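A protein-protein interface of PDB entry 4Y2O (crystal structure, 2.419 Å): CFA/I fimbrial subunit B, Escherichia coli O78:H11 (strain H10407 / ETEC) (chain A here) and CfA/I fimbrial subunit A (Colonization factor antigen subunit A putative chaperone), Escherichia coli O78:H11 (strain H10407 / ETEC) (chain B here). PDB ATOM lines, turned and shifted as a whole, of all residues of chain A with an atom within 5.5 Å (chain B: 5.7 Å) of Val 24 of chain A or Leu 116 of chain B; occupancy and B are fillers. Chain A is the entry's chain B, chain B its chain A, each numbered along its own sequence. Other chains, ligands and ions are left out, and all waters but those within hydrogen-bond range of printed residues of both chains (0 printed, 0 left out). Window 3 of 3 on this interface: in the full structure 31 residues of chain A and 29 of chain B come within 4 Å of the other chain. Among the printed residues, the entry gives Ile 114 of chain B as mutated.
Hydrophobic or aromatic side chains of chain A that line the printed part of chain B: Val 24, Val 133 and Val 134. Hydrophobic or aromatic side chains of chain B within 4 Å of the printed part of chain A: Ile 114, Leu 116 and Val 118. Along chain B the printed residues that touch a printed residue of chain A span positions 114 to 118. Among the printed residues, no Asp or Glu carboxylate lies within 4 Å of a Lys or Arg side-chain nitrogen of the other chain.
N of Gly 132 of chain A is in hydrogen-bond range of O of Glu 115 of chain B, at 3.4 Å. The backbone carbonyl oxygen (O) of Ser 117 of chain B is in hydrogen-bond range of the backbone NH (N) of Val 134 of chain A (3.0 Å). O of Gly 132 of chain A lies within hydrogen-bond range of N of Ser 117 of chain B. O of Ser 22 of chain A sits close to N of Val 118 of chain B (2.2 Å).
Ser 117 of chain B touches Ser 22 of chain A (CA to O, 2.9 Å). CA of Ala 23 of chain A touches CA of Ser 117 of chain B, 3.6 Å away. Val 24 of chain A touches Leu 116 of chain B (CG1 to O, 3.5 Å). Val 118 of chain B touches Val 24 of chain A (CG2 to CG1, 3.9 Å). Ile 114 of chain B touches Lys 25 of chain A. Leu 116 of chain B touches Gln 62 of chain A (CD1 to O, 3.7 Å). Ile 114 of chain B touches Ser 131 of chain A. Ser 131 of chain A touches Glu 115 of chain B. Leu 116 of chain B touches Val 133 of chain A. Val 118 of chain B touches Val 134 of chain A.
Of the printed residues of chain B, Val 24 of chain A touches Leu 116 (3.5 Å) and Val 118 (3.9 Å). Printed residues of chain B within 4 Å of Lys 25 of chain A: Ile 114. Leu 26 of chain A touches none of the printed residues of chain B. Printed residues of chain B within 4 Å of Gln 62 of chain A: Leu 116 (3.7 Å). Printed residues of chain B within 4 Å of Ser 131 of chain A: Ile 114 (3.4 Å) and Glu 115 (3.9 Å). Printed residues of chain B within 4 Å of Val 133 of chain A: Leu 116 and Ser 117. Of the printed residues of chain A, Glu 115 of chain B touches Ser 131 and Gly 132. The nearest printed residue of chain B that does not touch Val 24 of chain A is Ile 114 of chain B (4.02 Å). The nearest printed residue of chain A that does not touch Glu 115 of chain B is Ala 23 of chain A (4.03 Å).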
ATOM      1  N   SER A  22       6.829 -14.731  15.870  1.00  0.00           N
ATOM      2  CA  SER A  22       7.073 -14.029  14.626  1.00  0.00           C
ATOM      3  C   SER A  22       6.470 -14.776  13.450  1.00  0.00           C
ATOM      4  O   SER A  22       5.585 -14.266  12.784  1.00  0.00           O
ATOM      5  CB  SER A  22       8.570 -13.845  14.406  1.00  0.00           C
ATOM      6  OG  SER A  22       8.835 -13.365  13.100  1.00  0.00           O
ATOM      7  N   ALA A  23       6.952 -15.992  13.211  1.00  0.00           N
ATOM      8  CA  ALA A  23       6.511 -16.793  12.078  1.00  0.00           C
ATOM      9  C   ALA A  23       5.662 -17.970  12.486  1.00  0.00           C
ATOM     10  O   ALA A  23       5.777 -18.477  13.588  1.00  0.00           O
ATOM     11  CB  ALA A  23       7.687 -17.277  11.296  1.00  0.00           C
ATOM     12  N   VAL A  24       4.814 -18.404  11.567  1.00  0.00           N
ATOM     13  CA  VAL A  24       3.937 -19.534  11.807  1.00  0.00           C
ATOM     14  C   VAL A  24       3.760 -20.416  10.575  1.00  0.00           C
ATOM     15  O   VAL A  24       3.448 -19.927   9.492  1.00  0.00           O
ATOM     16  CB  VAL A  24       2.558 -19.075  12.268  1.00  0.00           C
ATOM     17  CG1 VAL A  24       2.140 -17.847  11.506  1.00  0.00           C
ATOM     18  CG2 VAL A  24       1.558 -20.173  12.047  1.00  0.00           C
ATOM     19  N   LYS A  25       3.953 -21.719  10.755  1.00  0.00           N
ATOM     20  CA  LYS A  25       3.681 -22.688   9.702  1.00  0.00           C
ATOM     21  C   LYS A  25       2.544 -23.632   9.996  1.00  0.00           C
ATOM     22  O   LYS A  25       2.522 -24.343  11.007  1.00  0.00           O
ATOM     23  CB  LYS A  25       4.908 -23.519   9.414  1.00  0.00           C
ATOM     24  CG  LYS A  25       5.962 -22.732   8.758  1.00  0.00           C
ATOM     25  CD  LYS A  25       7.275 -23.399   8.836  1.00  0.00           C
ATOM     26  CE  LYS A  25       8.125 -22.665   9.814  1.00  0.00           C
ATOM     27  NZ  LYS A  25       7.388 -22.422  11.075  1.00  0.00           N
ATOM     28  N   LEU A  26       1.614 -23.655   9.057  1.00  0.00           N
ATOM     29  CA  LEU A  26       0.566 -24.641   9.062  1.00  0.00           C
ATOM     30  C   LEU A  26       1.161 -25.947   8.595  1.00  0.00           C
ATOM     31  O   LEU A  26       1.930 -25.952   7.644  1.00  0.00           O
ATOM     32  CB  LEU A  26      -0.582 -24.210   8.165  1.00  0.00           C
ATOM     33  CG  LEU A  26      -1.659 -23.657   9.065  1.00  0.00           C
ATOM     34  CD1 LEU A  26      -2.172 -24.817   9.933  1.00  0.00           C
ATOM     35  CD2 LEU A  26      -1.085 -22.495   9.912  1.00  0.00           C
ATOM     36  N   TYR A  38      -4.259 -22.755  12.266  1.00  0.00           N
ATOM     37  CA  TYR A  38      -3.336 -22.423  13.342  1.00  0.00           C
ATOM     38  C   TYR A  38      -4.157 -21.727  14.383  1.00  0.00           C
ATOM     39  O   TYR A  38      -4.088 -20.520  14.525  1.00  0.00           O
ATOM     40  CB  TYR A  38      -2.211 -21.477  12.918  1.00  0.00           C
ATOM     41  CG  TYR A  38      -1.429 -20.845  14.082  1.00  0.00           C
ATOM     42  CD1 TYR A  38      -1.397 -21.432  15.348  1.00  0.00           C
ATOM     43  CD2 TYR A  38      -0.893 -19.570  13.962  1.00  0.00           C
ATOM     44  CE1 TYR A  38      -0.746 -20.834  16.393  1.00  0.00           C
ATOM     45  CE2 TYR A  38      -0.237 -18.969  15.004  1.00  0.00           C
ATOM     46  CZ  TYR A  38      -0.175 -19.592  16.226  1.00  0.00           C
ATOM     47  OH  TYR A  38       0.481 -18.983  17.277  1.00  0.00           O
ATOM     48  N   PRO A  61      -3.339 -10.179   3.125  1.00  0.00           N
ATOM     49  CA  PRO A  61      -2.103 -10.936   3.253  1.00  0.00           C
ATOM     50  C   PRO A  61      -1.938 -11.920   2.130  1.00  0.00           C
ATOM     51  O   PRO A  61      -2.914 -12.400   1.569  1.00  0.00           O
ATOM     52  CB  PRO A  61      -2.274 -11.644   4.580  1.00  0.00           C
ATOM     53  CG  PRO A  61      -3.717 -11.827   4.701  1.00  0.00           C
ATOM     54  CD  PRO A  61      -4.344 -10.622   4.095  1.00  0.00           C
ATOM     55  N   GLN A  62      -0.699 -12.209   1.783  1.00  0.00           N
ATOM     56  CA  GLN A  62      -0.467 -13.051   0.636  1.00  0.00           C
ATOM     57  C   GLN A  62       0.598 -14.072   0.915  1.00  0.00           C
ATOM     58  O   GLN A  62       1.550 -13.795   1.638  1.00  0.00           O
ATOM     59  CB  GLN A  62      -0.036 -12.206  -0.564  1.00  0.00           C
ATOM     60  CG  GLN A  62       1.230 -11.313  -0.366  1.00  0.00           C
ATOM     61  CD  GLN A  62       1.113 -10.205   0.686  1.00  0.00           C
ATOM     62  OE1 GLN A  62       0.157 -10.138   1.438  1.00  0.00           O
ATOM     63  NE2 GLN A  62       2.101  -9.327   0.723  1.00  0.00           N
ATOM     64  N   ALA A  63       0.474 -15.242   0.307  1.00  0.00           N
ATOM     65  CA  ALA A  63       1.615 -16.114   0.261  1.00  0.00           C
ATOM     66  C   ALA A  63       2.433 -15.485  -0.822  1.00  0.00           C
ATOM     67  O   ALA A  63       1.993 -15.391  -1.963  1.00  0.00           O
ATOM     68  CB  ALA A  63       1.236 -17.521  -0.069  1.00  0.00           C
ATOM     69  N   ILE A  75      -5.958 -16.502   2.278  1.00  0.00           N
ATOM     70  CA  ILE A  75      -5.792 -16.684   3.712  1.00  0.00           C
ATOM     71  C   ILE A  75      -6.926 -16.033   4.466  1.00  0.00           C
ATOM     72  O   ILE A  75      -7.146 -14.841   4.323  1.00  0.00           O
ATOM     73  CB  ILE A  75      -4.507 -16.077   4.222  1.00  0.00           C
ATOM     74  CG1 ILE A  75      -3.320 -16.495   3.360  1.00  0.00           C
ATOM     75  CG2 ILE A  75      -4.305 -16.488   5.650  1.00  0.00           C
ATOM     76  CD1 ILE A  75      -2.999 -15.540   2.232  1.00  0.00           C
ATOM     77  N   ILE A 114      -6.435 -18.346  12.257  1.00  0.00           N
ATOM     78  CA  ILE A 114      -5.948 -18.079  10.939  1.00  0.00           C
ATOM     79  C   ILE A 114      -6.135 -19.336  10.125  1.00  0.00           C
ATOM     80  O   ILE A 114      -5.522 -20.359  10.401  1.00  0.00           O
ATOM     81  CB  ILE A 114      -4.508 -17.657  10.955  1.00  0.00           C
ATOM     82  CG1 ILE A 114      -3.883 -17.909   9.594  1.00  0.00           C
ATOM     83  CG2 ILE A 114      -3.790 -18.408  12.012  1.00  0.00           C
ATOM     84  CD1 ILE A 114      -2.542 -17.310   9.439  1.00  0.00           C
ATOM     85  N   SER A 131       5.957 -17.846   0.291  1.00  0.00           N
ATOM     86  CA  SER A 131       6.436 -17.115   1.490  1.00  0.00           C
ATOM     87  C   SER A 131       5.525 -15.972   1.921  1.00  0.00           C
ATOM     88  O   SER A 131       4.375 -15.935   1.551  1.00  0.00           O
ATOM     89  CB  SER A 131       7.840 -16.536   1.279  1.00  0.00           C
ATOM     90  OG  SER A 131       8.115 -15.525   2.213  1.00  0.00           O
ATOM     91  N   GLY A 132       5.934 -15.173   2.892  1.00  0.00           N
ATOM     92  CA  GLY A 132       5.030 -14.085   3.201  1.00  0.00           C
ATOM     93  C   GLY A 132       5.017 -13.513   4.612  1.00  0.00           C
ATOM     94  O   GLY A 132       5.828 -13.844   5.475  1.00  0.00           O
ATOM     95  N   VAL A 133       4.038 -12.623   4.799  1.00  0.00           N
ATOM     96  CA  VAL A 133       3.755 -11.966   6.061  1.00  0.00           C
ATOM     97  C   VAL A 133       2.273 -11.620   6.253  1.00  0.00           C
ATOM     98  O   VAL A 133       1.511 -11.499   5.295  1.00  0.00           O
ATOM     99  CB  VAL A 133       4.522 -10.643   6.208  1.00  0.00           C
ATOM    100  CG1 VAL A 133       5.982 -10.915   6.387  1.00  0.00           C
ATOM    101  CG2 VAL A 133       4.281  -9.770   5.027  1.00  0.00           C
ATOM    102  N   VAL A 134       1.885 -11.454   7.509  1.00  0.00           N
ATOM    103  CA  VAL A 134       0.572 -10.947   7.851  1.00  0.00           C
ATOM    104  C   VAL A 134       0.678  -9.842   8.877  1.00  0.00           C
ATOM    105  O   VAL A 134       1.009 -10.084  10.029  1.00  0.00           O
ATOM    106  CB  VAL A 134      -0.335 -12.015   8.417  1.00  0.00           C
ATOM    107  CG1 VAL A 134      -1.603 -11.387   8.926  1.00  0.00           C
ATOM    108  CG2 VAL A 134      -0.666 -13.001   7.376  1.00  0.00           C
ATOM    109  N   ILE B 114       6.116 -22.916   4.156  1.00  0.00           N
ATOM    110  CA  ILE B 114       6.730 -21.596   4.321  1.00  0.00           C
ATOM    111  C   ILE B 114       6.558 -20.898   5.638  1.00  0.00           C
ATOM    112  O   ILE B 114       5.679 -21.228   6.414  1.00  0.00           O
ATOM    113  CB  ILE B 114       6.200 -20.564   3.296  1.00  0.00           C
ATOM    114  CG1 ILE B 114       4.769 -20.874   2.859  1.00  0.00           C
ATOM    115  CG2 ILE B 114       7.207 -20.379   2.144  1.00  0.00           C
ATOM    116  CD1 ILE B 114       3.735 -20.588   3.867  1.00  0.00           C
ATOM    117  N   GLU B 115       7.344 -19.842   5.811  1.00  0.00           N
ATOM    118  CA  GLU B 115       7.122 -18.929   6.909  1.00  0.00           C
ATOM    119  C   GLU B 115       6.368 -17.647   6.520  1.00  0.00           C
ATOM    120  O   GLU B 115       6.787 -16.874   5.661  1.00  0.00           O
ATOM    121  CB  GLU B 115       8.447 -18.593   7.565  1.00  0.00           C
ATOM    122  CG  GLU B 115       9.491 -18.028   6.639  1.00  0.00           C
ATOM    123  CD  GLU B 115       9.765 -16.581   6.947  1.00  0.00           C
ATOM    124  OE1 GLU B 115      10.936 -16.172   6.909  1.00  0.00           O
ATOM    125  OE2 GLU B 115       8.796 -15.858   7.236  1.00  0.00           O
ATOM    126  N   LEU B 116       5.232 -17.457   7.181  1.00  0.00           N
ATOM    127  CA  LEU B 116       4.424 -16.264   7.036  1.00  0.00           C
ATOM    128  C   LEU B 116       4.430 -15.548   8.363  1.00  0.00           C
ATOM    129  O   LEU B 116       3.493 -15.673   9.151  1.00  0.00           O
ATOM    130  CB  LEU B 116       3.012 -16.626   6.609  1.00  0.00           C
ATOM    131  CG  LEU B 116       1.900 -15.590   6.542  1.00  0.00           C
ATOM    132  CD1 LEU B 116       1.690 -15.005   5.153  1.00  0.00           C
ATOM    133  CD2 LEU B 116       0.663 -16.293   7.025  1.00  0.00           C
ATOM    134  N   SER B 117       5.507 -14.805   8.594  1.00  0.00           N
ATOM    135  CA  SER B 117       5.720 -14.107   9.846  1.00  0.00           C
ATOM    136  C   SER B 117       4.592 -13.161  10.165  1.00  0.00           C
ATOM    137  O   SER B 117       4.057 -12.510   9.285  1.00  0.00           O
ATOM    138  CB  SER B 117       7.039 -13.355   9.820  1.00  0.00           C
ATOM    139  OG  SER B 117       7.216 -12.682   8.591  1.00  0.00           O
ATOM    140  N   VAL B 118       4.235 -13.096  11.438  1.00  0.00           N
ATOM    141  CA  VAL B 118       3.125 -12.277  11.866  1.00  0.00           C
ATOM    142  C   VAL B 118       3.590 -10.976  12.486  1.00  0.00           C
ATOM    143  O   VAL B 118       4.264 -10.970  13.506  1.00  0.00           O
ATOM    144  CB  VAL B 118       2.261 -13.022  12.846  1.00  0.00           C
ATOM    145  CG1 VAL B 118       1.311 -12.087  13.508  1.00  0.00           C
ATOM    146  CG2 VAL B 118       1.514 -14.083  12.121  1.00  0.00           C
